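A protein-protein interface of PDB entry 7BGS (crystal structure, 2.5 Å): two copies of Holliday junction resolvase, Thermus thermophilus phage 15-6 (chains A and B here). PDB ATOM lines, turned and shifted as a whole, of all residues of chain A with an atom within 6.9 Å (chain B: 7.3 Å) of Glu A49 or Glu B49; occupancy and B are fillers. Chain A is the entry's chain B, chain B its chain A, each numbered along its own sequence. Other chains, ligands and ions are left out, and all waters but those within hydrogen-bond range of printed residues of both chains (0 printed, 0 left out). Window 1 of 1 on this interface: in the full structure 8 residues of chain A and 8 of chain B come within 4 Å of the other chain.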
ATOM      1  N   TRP A  25       1.618 -21.847  25.897  1.00  0.00           N
ATOM      2  CA  TRP A  25       1.837 -20.542  25.275  1.00  0.00           C
ATOM      3  C   TRP A  25       1.465 -20.517  23.770  1.00  0.00           C
ATOM      4  O   TRP A  25       1.216 -21.560  23.185  1.00  0.00           O
ATOM      5  CB  TRP A  25       3.272 -20.050  25.524  1.00  0.00           C
ATOM      6  CG  TRP A  25       4.328 -20.839  24.823  1.00  0.00           C
ATOM      7  CD1 TRP A  25       4.861 -20.583  23.597  1.00  0.00           C
ATOM      8  CD2 TRP A  25       4.998 -22.007  25.319  1.00  0.00           C
ATOM      9  NE1 TRP A  25       5.808 -21.528  23.289  1.00  0.00           N
ATOM     10  CE2 TRP A  25       5.929 -22.401  24.341  1.00  0.00           C
ATOM     11  CE3 TRP A  25       4.896 -22.766  26.493  1.00  0.00           C
ATOM     12  CZ2 TRP A  25       6.805 -23.472  24.533  1.00  0.00           C
ATOM     13  CZ3 TRP A  25       5.691 -23.886  26.632  1.00  0.00           C
ATOM     14  CH2 TRP A  25       6.634 -24.227  25.662  1.00  0.00           C
ATOM     15  N   VAL A  27       2.212 -19.545  19.596  1.00  0.00           N
ATOM     16  CA  VAL A  27       3.186 -19.309  18.520  1.00  0.00           C
ATOM     17  C   VAL A  27       2.443 -18.974  17.209  1.00  0.00           C
ATOM     18  O   VAL A  27       1.726 -19.821  16.664  1.00  0.00           O
ATOM     19  CB  VAL A  27       4.153 -20.504  18.321  1.00  0.00           C
ATOM     20  CG1 VAL A  27       5.116 -20.248  17.165  1.00  0.00           C
ATOM     21  CG2 VAL A  27       4.912 -20.837  19.603  1.00  0.00           C
ATOM     22  N   LEU A  29       3.464 -18.430  13.866  1.00  0.00           N
ATOM     23  CA  LEU A  29       3.917 -19.189  12.684  1.00  0.00           C
ATOM     24  C   LEU A  29       3.488 -18.552  11.353  1.00  0.00           C
ATOM     25  O   LEU A  29       4.329 -18.290  10.495  1.00  0.00           O
ATOM     26  CB  LEU A  29       3.518 -20.676  12.760  1.00  0.00           C
ATOM     27  CG  LEU A  29       4.452 -21.582  13.572  1.00  0.00           C
ATOM     28  CD1 LEU A  29       3.851 -22.974  13.749  1.00  0.00           C
ATOM     29  CD2 LEU A  29       5.824 -21.670  12.931  1.00  0.00           C
ATOM     30  N   VAL A  41      -0.385 -23.469  19.034  1.00  0.00           N
ATOM     31  CA  VAL A  41      -0.259 -23.352  20.502  1.00  0.00           C
ATOM     32  C   VAL A  41       0.767 -24.408  21.032  1.00  0.00           C
ATOM     33  O   VAL A  41       0.806 -25.493  20.485  1.00  0.00           O
ATOM     34  CB  VAL A  41      -1.669 -23.478  21.174  1.00  0.00           C
ATOM     35  CG1 VAL A  41      -1.595 -24.005  22.606  1.00  0.00           C
ATOM     36  CG2 VAL A  41      -2.400 -22.148  21.135  1.00  0.00           C
ATOM     37  N   ARG A  42       1.588 -24.111  22.059  1.00  0.00           N
ATOM     38  CA  ARG A  42       2.527 -25.110  22.604  1.00  0.00           C
ATOM     39  C   ARG A  42       2.171 -25.515  24.036  1.00  0.00           C
ATOM     40  O   ARG A  42       1.731 -24.663  24.799  1.00  0.00           O
ATOM     41  CB  ARG A  42       4.001 -24.634  22.542  1.00  0.00           C
ATOM     42  CG  ARG A  42       4.491 -24.192  21.170  1.00  0.00           C
ATOM     43  CD  ARG A  42       4.287 -25.261  20.115  1.00  0.00           C
ATOM     44  NE  ARG A  42       5.331 -25.184  19.100  1.00  0.00           N
ATOM     45  CZ  ARG A  42       5.239 -24.481  17.979  1.00  0.00           C
ATOM     46  NH1 ARG A  42       4.133 -23.807  17.699  1.00  0.00           N
ATOM     47  NH2 ARG A  42       6.254 -24.448  17.125  1.00  0.00           N
ATOM     48  N   VAL A  43       2.366 -26.801  24.409  1.00  0.00           N
ATOM     49  CA  VAL A  43       2.070 -27.254  25.771  1.00  0.00           C
ATOM     50  C   VAL A  43       3.210 -28.151  26.305  1.00  0.00           C
ATOM     51  O   VAL A  43       3.872 -28.858  25.539  1.00  0.00           O
ATOM     52  CB  VAL A  43       0.643 -27.899  25.908  1.00  0.00           C
ATOM     53  CG1 VAL A  43       0.557 -29.264  25.243  1.00  0.00           C
ATOM     54  CG2 VAL A  43       0.165 -27.962  27.360  1.00  0.00           C
ATOM     55  N   MET A  44       3.461 -28.093  27.617  1.00  0.00           N
ATOM     56  CA  MET A  44       4.487 -28.919  28.240  1.00  0.00           C
ATOM     57  C   MET A  44       3.824 -30.128  28.874  1.00  0.00           C
ATOM     58  O   MET A  44       2.895 -29.954  29.671  1.00  0.00           O
ATOM     59  CB  MET A  44       5.231 -28.117  29.296  1.00  0.00           C
ATOM     60  CG  MET A  44       6.027 -26.965  28.715  1.00  0.00           C
ATOM     61  SD  MET A  44       7.508 -27.531  27.563  1.00  0.00           S
ATOM     62  CE  MET A  44       8.699 -28.410  28.922  1.00  0.00           C
ATOM     63  N   LEU A  45       4.257 -31.352  28.478  1.00  0.00           N
ATOM     64  CA  LEU A  45       3.731 -32.635  28.962  1.00  0.00           C
ATOM     65  C   LEU A  45       4.885 -33.538  29.260  1.00  0.00           C
ATOM     66  O   LEU A  45       5.584 -33.952  28.330  1.00  0.00           O
ATOM     67  CB  LEU A  45       2.879 -33.333  27.897  1.00  0.00           C
ATOM     68  CG  LEU A  45       1.600 -32.646  27.474  1.00  0.00           C
ATOM     69  CD1 LEU A  45       1.009 -33.323  26.260  1.00  0.00           C
ATOM     70  CD2 LEU A  45       0.619 -32.626  28.604  1.00  0.00           C
ATOM     71  N   ALA A  46       5.084 -33.886  30.545  1.00  0.00           N
ATOM     72  CA  ALA A  46       6.198 -34.736  31.019  1.00  0.00           C
ATOM     73  C   ALA A  46       7.560 -34.145  30.721  1.00  0.00           C
ATOM     74  O   ALA A  46       8.542 -34.879  30.609  1.00  0.00           O
ATOM     75  CB  ALA A  46       6.099 -36.143  30.457  1.00  0.00           C
ATOM     76  N   GLY A  47       7.646 -32.820  30.639  1.00  0.00           N
ATOM     77  CA  GLY A  47       8.926 -32.162  30.374  1.00  0.00           C
ATOM     78  C   GLY A  47       9.265 -32.071  28.897  1.00  0.00           C
ATOM     79  O   GLY A  47      10.423 -31.835  28.559  1.00  0.00           O
ATOM     80  N   GLN A  48       8.259 -32.249  28.005  1.00  0.00           N
ATOM     81  CA  GLN A  48       8.409 -32.195  26.552  1.00  0.00           C
ATOM     82  C   GLN A  48       7.416 -31.204  25.955  1.00  0.00           C
ATOM     83  O   GLN A  48       6.266 -31.148  26.370  1.00  0.00           O
ATOM     84  CB  GLN A  48       8.180 -33.579  25.931  1.00  0.00           C
ATOM     85  CG  GLN A  48       9.286 -34.570  26.267  1.00  0.00           C
ATOM     86  CD  GLN A  48       9.371 -35.700  25.269  1.00  0.00           C
ATOM     87  OE1 GLN A  48       8.374 -36.064  24.632  1.00  0.00           O
ATOM     88  NE2 GLN A  48      10.560 -36.263  25.111  1.00  0.00           N
ATOM     89  N   GLU A  49       7.851 -30.438  24.956  1.00  0.00           N
ATOM     90  CA  GLU A  49       6.997 -29.461  24.293  1.00  0.00           C
ATOM     91  C   GLU A  49       6.206 -30.143  23.181  1.00  0.00           C
ATOM     92  O   GLU A  49       6.753 -30.966  22.447  1.00  0.00           O
ATOM     93  CB  GLU A  49       7.847 -28.326  23.716  1.00  0.00           C
ATOM     94  CG  GLU A  49       7.031 -27.202  23.112  1.00  0.00           C
ATOM     95  CD  GLU A  49       7.883 -26.245  22.310  1.00  0.00           C
ATOM     96  OE1 GLU A  49       8.977 -25.871  22.789  1.00  0.00           O
ATOM     97  OE2 GLU A  49       7.468 -25.894  21.184  1.00  0.00           O
ATOM     98  N   HIS A  50       4.924 -29.838  23.079  1.00  0.00           N
ATOM     99  CA  HIS A  50       4.063 -30.404  22.058  1.00  0.00           C
ATOM    100  C   HIS A  50       3.273 -29.327  21.349  1.00  0.00           C
ATOM    101  O   HIS A  50       2.732 -28.433  22.003  1.00  0.00           O
ATOM    102  CB  HIS A  50       3.083 -31.396  22.679  1.00  0.00           C
ATOM    103  CG  HIS A  50       3.744 -32.534  23.373  1.00  0.00           C
ATOM    104  ND1 HIS A  50       4.245 -33.612  22.671  1.00  0.00           N
ATOM    105  CD2 HIS A  50       3.986 -32.718  24.690  1.00  0.00           C
ATOM    106  CE1 HIS A  50       4.759 -34.421  23.579  1.00  0.00           C
ATOM    107  NE2 HIS A  50       4.624 -33.924  24.810  1.00  0.00           N
ATOM    108  N   ARG A  51       3.188 -29.417  20.014  1.00  0.00           N
ATOM    109  CA  ARG A  51       2.399 -28.475  19.234  1.00  0.00           C
ATOM    110  C   ARG A  51       0.952 -28.867  19.399  1.00  0.00           C
ATOM    111  O   ARG A  51       0.634 -30.046  19.270  1.00  0.00           O
ATOM    112  CB  ARG A  51       2.693 -28.614  17.742  1.00  0.00           C
ATOM    113  CG  ARG A  51       4.042 -28.169  17.273  1.00  0.00           C
ATOM    114  CD  ARG A  51       4.301 -28.829  15.941  1.00  0.00           C
ATOM    115  NE  ARG A  51       4.388 -30.284  16.099  1.00  0.00           N
ATOM    116  CZ  ARG A  51       4.698 -31.125  15.116  1.00  0.00           C
ATOM    117  NH1 ARG A  51       4.908 -30.672  13.886  1.00  0.00           N
ATOM    118  NH2 ARG A  51       4.824 -32.423  15.361  1.00  0.00           N
ATOM    119  N   TRP B  25      13.071 -17.846  25.076  1.00  0.00           N
ATOM    120  CA  TRP B  25      12.710 -18.407  26.374  1.00  0.00           C
ATOM    121  C   TRP B  25      13.386 -19.748  26.652  1.00  0.00           C
ATOM    122  O   TRP B  25      13.982 -20.346  25.765  1.00  0.00           O
ATOM    123  CB  TRP B  25      11.167 -18.487  26.535  1.00  0.00           C
ATOM    124  CG  TRP B  25      10.508 -19.497  25.648  1.00  0.00           C
ATOM    125  CD1 TRP B  25      10.216 -20.790  25.957  1.00  0.00           C
ATOM    126  CD2 TRP B  25      10.066 -19.298  24.298  1.00  0.00           C
ATOM    127  NE1 TRP B  25       9.616 -21.408  24.889  1.00  0.00           N
ATOM    128  CE2 TRP B  25       9.491 -20.507  23.863  1.00  0.00           C
ATOM    129  CE3 TRP B  25      10.065 -18.204  23.431  1.00  0.00           C
ATOM    130  CZ2 TRP B  25       8.933 -20.652  22.595  1.00  0.00           C
ATOM    131  CZ3 TRP B  25       9.545 -18.359  22.169  1.00  0.00           C
ATOM    132  CH2 TRP B  25       8.981 -19.569  21.761  1.00  0.00           C
ATOM    133  N   VAL B  27      12.566 -23.595  28.196  1.00  0.00           N
ATOM    134  CA  VAL B  27      11.409 -24.441  28.525  1.00  0.00           C
ATOM    135  C   VAL B  27      11.542 -25.107  29.891  1.00  0.00           C
ATOM    136  O   VAL B  27      12.597 -25.635  30.233  1.00  0.00           O
ATOM    137  CB  VAL B  27      10.995 -25.472  27.439  1.00  0.00           C
ATOM    138  CG1 VAL B  27      10.001 -24.863  26.464  1.00  0.00           C
ATOM    139  CG2 VAL B  27      12.196 -26.050  26.706  1.00  0.00           C
ATOM    140  N   SER B  39      18.674 -28.725  23.726  1.00  0.00           N
ATOM    141  CA  SER B  39      17.843 -27.627  23.247  1.00  0.00           C
ATOM    142  C   SER B  39      16.768 -27.262  24.262  1.00  0.00           C
ATOM    143  O   SER B  39      15.636 -27.745  24.192  1.00  0.00           O
ATOM    144  CB  SER B  39      17.218 -27.967  21.896  1.00  0.00           C
ATOM    145  OG  SER B  39      18.213 -28.081  20.890  1.00  0.00           O
ATOM    146  N   ASP B  40      17.141 -26.414  25.220  1.00  0.00           N
ATOM    147  CA  ASP B  40      16.239 -25.906  26.256  1.00  0.00           C
ATOM    148  C   ASP B  40      15.774 -24.472  25.939  1.00  0.00           C
ATOM    149  O   ASP B  40      14.776 -24.029  26.487  1.00  0.00           O
ATOM    150  CB  ASP B  40      16.951 -25.940  27.610  1.00  0.00           C
ATOM    151  CG  ASP B  40      16.041 -25.993  28.828  1.00  0.00           C
ATOM    152  OD1 ASP B  40      14.878 -26.441  28.686  1.00  0.00           O
ATOM    153  OD2 ASP B  40      16.505 -25.611  29.931  1.00  0.00           O
ATOM    154  N   VAL B  41      16.490 -23.761  25.045  1.00  0.00           N
ATOM    155  CA  VAL B  41      16.204 -22.405  24.611  1.00  0.00           C
ATOM    156  C   VAL B  41      15.400 -22.402  23.293  1.00  0.00           C
ATOM    157  O   VAL B  41      15.665 -23.197  22.395  1.00  0.00           O
ATOM    158  CB  VAL B  41      17.543 -21.622  24.485  1.00  0.00           C
ATOM    159  CG1 VAL B  41      17.326 -20.197  23.997  1.00  0.00           C
ATOM    160  CG2 VAL B  41      18.299 -21.632  25.806  1.00  0.00           C
ATOM    161  N   ARG B  42      14.409 -21.523  23.191  1.00  0.00           N
ATOM    162  CA  ARG B  42      13.635 -21.364  21.975  1.00  0.00           C
ATOM    163  C   ARG B  42      13.733 -19.916  21.541  1.00  0.00           C
ATOM    164  O   ARG B  42      13.662 -19.027  22.382  1.00  0.00           O
ATOM    165  CB  ARG B  42      12.153 -21.691  22.208  1.00  0.00           C
ATOM    166  CG  ARG B  42      11.835 -23.063  22.778  1.00  0.00           C
ATOM    167  CD  ARG B  42      12.311 -24.171  21.860  1.00  0.00           C
ATOM    168  NE  ARG B  42      11.687 -25.451  22.186  1.00  0.00           N
ATOM    169  CZ  ARG B  42      12.242 -26.385  22.951  1.00  0.00           C
ATOM    170  NH1 ARG B  42      13.451 -26.196  23.471  1.00  0.00           N
ATOM    171  NH2 ARG B  42      11.596 -27.519  23.199  1.00  0.00           N
ATOM    172  N   VAL B  43      13.841 -19.663  20.237  1.00  0.00           N
ATOM    173  CA  VAL B  43      13.868 -18.290  19.727  1.00  0.00           C
ATOM    174  C   VAL B  43      12.834 -18.127  18.586  1.00  0.00           C
ATOM    175  O   VAL B  43      12.570 -19.069  17.834  1.00  0.00           O
ATOM    176  CB  VAL B  43      15.300 -17.808  19.367  1.00  0.00           C
ATOM    177  CG1 VAL B  43      15.818 -18.472  18.102  1.00  0.00           C
ATOM    178  CG2 VAL B  43      15.375 -16.293  19.258  1.00  0.00           C
ATOM    179  N   MET B  44      12.176 -16.968  18.521  1.00  0.00           N
ATOM    180  CA  MET B  44      11.192 -16.697  17.482  1.00  0.00           C
ATOM    181  C   MET B  44      11.816 -15.867  16.359  1.00  0.00           C
ATOM    182  O   MET B  44      12.194 -14.713  16.573  1.00  0.00           O
ATOM    183  CB  MET B  44       9.983 -15.984  18.078  1.00  0.00           C
ATOM    184  CG  MET B  44       9.177 -16.869  19.006  1.00  0.00           C
ATOM    185  SD  MET B  44       7.867 -17.996  18.079  1.00  0.00           S
ATOM    186  CE  MET B  44       6.806 -16.594  17.332  1.00  0.00           C
ATOM    187  N   LEU B  45      11.962 -16.475  15.178  1.00  0.00           N
ATOM    188  CA  LEU B  45      12.509 -15.817  13.993  1.00  0.00           C
ATOM    189  C   LEU B  45      11.430 -15.780  12.924  1.00  0.00           C
ATOM    190  O   LEU B  45      10.874 -16.826  12.558  1.00  0.00           O
ATOM    191  CB  LEU B  45      13.747 -16.556  13.482  1.00  0.00           C
ATOM    192  CG  LEU B  45      14.937 -16.548  14.430  1.00  0.00           C
ATOM    193  CD1 LEU B  45      16.013 -17.487  13.954  1.00  0.00           C
ATOM    194  CD2 LEU B  45      15.453 -15.147  14.630  1.00  0.00           C
ATOM    195  N   ALA B  46      11.075 -14.565  12.473  1.00  0.00           N
ATOM    196  CA  ALA B  46       9.986 -14.332  11.511  1.00  0.00           C
ATOM    197  C   ALA B  46       8.676 -14.978  11.914  1.00  0.00           C
ATOM    198  O   ALA B  46       7.853 -15.324  11.046  1.00  0.00           O
ATOM    199  CB  ALA B  46      10.378 -14.770  10.108  1.00  0.00           C
ATOM    200  N   GLY B  47       8.461 -15.122  13.220  1.00  0.00           N
ATOM    201  CA  GLY B  47       7.217 -15.718  13.702  1.00  0.00           C
ATOM    202  C   GLY B  47       7.244 -17.233  13.749  1.00  0.00           C
ATOM    203  O   GLY B  47       6.193 -17.845  13.841  1.00  0.00           O
ATOM    204  N   GLN B  48       8.443 -17.849  13.714  1.00  0.00           N
ATOM    205  CA  GLN B  48       8.629 -19.296  13.759  1.00  0.00           C
ATOM    206  C   GLN B  48       9.505 -19.682  14.945  1.00  0.00           C
ATOM    207  O   GLN B  48      10.499 -19.000  15.206  1.00  0.00           O
ATOM    208  CB  GLN B  48       9.279 -19.792  12.462  1.00  0.00           C
ATOM    209  CG  GLN B  48       8.348 -19.684  11.259  1.00  0.00           C
ATOM    210  CD  GLN B  48       8.681 -20.671  10.167  1.00  0.00           C
ATOM    211  OE1 GLN B  48       9.739 -21.314  10.150  1.00  0.00           O
ATOM    212  NE2 GLN B  48       7.782 -20.813   9.225  1.00  0.00           N
ATOM    213  N   GLU B  49       9.129 -20.755  15.668  1.00  0.00           N
ATOM    214  CA  GLU B  49       9.871 -21.219  16.838  1.00  0.00           C
ATOM    215  C   GLU B  49      11.055 -22.137  16.469  1.00  0.00           C
ATOM    216  O   GLU B  49      10.851 -23.138  15.773  1.00  0.00           O
ATOM    217  CB  GLU B  49       8.942 -21.905  17.841  1.00  0.00           C
ATOM    218  CG  GLU B  49       9.661 -22.254  19.133  1.00  0.00           C
ATOM    219  CD  GLU B  49       9.159 -23.512  19.809  1.00  0.00           C
ATOM    220  OE1 GLU B  49       8.048 -23.467  20.382  1.00  0.00           O
ATOM    221  OE2 GLU B  49       9.876 -24.540  19.771  1.00  0.00           O
ATOM    222  N   HIS B  50      12.285 -21.787  16.939  1.00  0.00           N
ATOM    223  CA  HIS B  50      13.509 -22.542  16.659  1.00  0.00           C
ATOM    224  C   HIS B  50      14.231 -22.951  17.930  1.00  0.00           C
ATOM    225  O   HIS B  50      14.411 -22.139  18.832  1.00  0.00           O
ATOM    226  CB  HIS B  50      14.487 -21.728  15.792  1.00  0.00           C
ATOM    227  CG  HIS B  50      13.898 -21.283  14.495  1.00  0.00           C
ATOM    228  ND1 HIS B  50      13.780 -22.147  13.421  1.00  0.00           N
ATOM    229  CD2 HIS B  50      13.384 -20.082  14.150  1.00  0.00           C
ATOM    230  CE1 HIS B  50      13.203 -21.446  12.460  1.00  0.00           C
ATOM    231  NE2 HIS B  50      12.956 -20.194  12.850  1.00  0.00           N
ATOM    232  N   ARG B  51      14.654 -24.217  17.988  1.00  0.00           N
ATOM    233  CA  ARG B  51      15.418 -24.746  19.097  1.00  0.00           C
ATOM    234  C   ARG B  51      16.825 -24.203  18.957  1.00  0.00           C
ATOM    235  O   ARG B  51      17.406 -24.259  17.866  1.00  0.00           O
ATOM    236  CB  ARG B  51      15.563 -26.263  18.987  1.00  0.00           C
ATOM    237  CG  ARG B  51      14.312 -27.084  19.166  1.00  0.00           C
ATOM    238  CD  ARG B  51      14.457 -28.422  18.438  1.00  0.00           C
ATOM    239  NE  ARG B  51      14.744 -28.209  17.019  1.00  0.00           N
ATOM    240  CZ  ARG B  51      14.836 -29.164  16.107  1.00  0.00           C
ATOM    241  NH1 ARG B  51      15.135 -28.859  14.850  1.00  0.00           N
ATOM    242  NH2 ARG B  51      14.637 -30.433  16.441  1.00  0.00           N
ATOM    243  N   ILE B 114      20.115 -24.120  15.218  1.00  0.00           N
ATOM    244  CA  ILE B 114      20.898 -23.009  15.732  1.00  0.00           C
ATOM    245  C   ILE B 114      21.742 -23.519  16.892  1.00  0.00           C
ATOM    246  O   ILE B 114      21.252 -24.284  17.727  1.00  0.00           O
ATOM    247  CB  ILE B 114      19.975 -21.845  16.187  1.00  0.00           C
ATOM    248  CG1 ILE B 114      18.974 -21.464  15.081  1.00  0.00           C
ATOM    249  CG2 ILE B 114      20.794 -20.629  16.656  1.00  0.00           C
ATOM    250  CD1 ILE B 114      17.926 -20.498  15.502  1.00  0.00           C
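The side-chain carboxylate of Glu B49 lies close to the side-chain carboxylate of Glu A49.
NE of Arg A42 lies within salt-bridge range of OE1 of Glu B49 (3.5 Å).
NE of Arg B42 is in salt-bridge range of OE1 of Glu A49, at 2.8 Å.
The backbone NH of Leu A29 lies within hydrogen-bond range of the backbone carbonyl oxygen of Gly B47 (2.8 Å).
Of the printed residues of chain B, Val A27 touches Met B44.
Val A41 touches none of the printed residues of chain B.
Ala A46 touches none of the printed residues of chain B.
Glu A49 touches three residues of chain B.
Of the printed residues of chain A, Arg B42 touches Glu A49 (2.8 Å).
Of chain A, only Arg A42 (3.5 Å) and Glu A49 (2.6 Å) come within 4 Å of Glu B49.
The nearest residue of chain B that does not touch Glu A49 is Trp B25 (5.0 Å).
The nearest printed residue of chain A that does not touch Glu B49 is Trp A25 (4.2 Å).
OE2 of Glu B49 lies within salt-bridge range of NE of Arg B42, at 3.2 Å.
The backbone NH (N) of Arg A42 lies within hydrogen-bond range of the backbone carbonyl oxygen (O) of Trp A25 (2.8 Å).
The backbone NH (N) of Val B27 sits at hydrogen-bond distance from the backbone carbonyl oxygen (O) of Asp B40, at 2.8 Å.
The side-chain carboxylate (OE2) of Glu A49 is in salt-bridge range of the guanidinium group (NE) of Arg A42, 3.1 Å away.
O of Trp B25 sits at hydrogen-bond distance from N of Arg B42 (2.9 Å).
O of Ser B39 lies within hydrogen-bond range of NH1 of Arg B42.
Printed residues of chain A that touch a printed residue of chain B: Trp A25, Val A27, Leu A29, Arg A42, Met A44 and Glu A49.
Of the 16 printed residues of chain B, 7 touch a printed residue of chain A.
Printed residues of chain B that touch a printed residue of chain A: Trp B25, Val B27, Arg B42, Met B44, Gly B47, Gln B48 and Glu B49.
Hydrophobic or aromatic side chains of chain B within 4 Å of the printed part of chain A: Trp B25, Val B27 and Met B44.
Among the printed residues, 10 pairs touch across the chains.
Among the printed residues, Asp or Glu carboxylates within 4 Å of a Lys or Arg side-chain nitrogen of the other chain: Arg A42 with Glu B49 (3.5 Å) and Glu A49 with Arg B42 (2.8 Å).
Among the printed residues, pairs that only touch across the chains: Trp A25 with Trp B25, Trp A25 with Val B27, Leu A29 with Gln B48, Val A27 with Met B44, Met A44 with Val B27 and Glu A49 with Val B27.
Trp A25 touches Val B27, but with the chains exchanged Val A27 does not touch Trp B25 (4.8 Å).
Val A27 touches Met B44, and with the chains exchanged Met A44 touches Val B27.
Arg A42 touches Glu B49, and with the chains exchanged Glu A49 touches Arg B42.
Glu B49 touches its own counterpart, Glu A49.
Of the 10 pairs that touch across the chains among the printed residues, 6 have their exchanged pair printed and touching as well.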
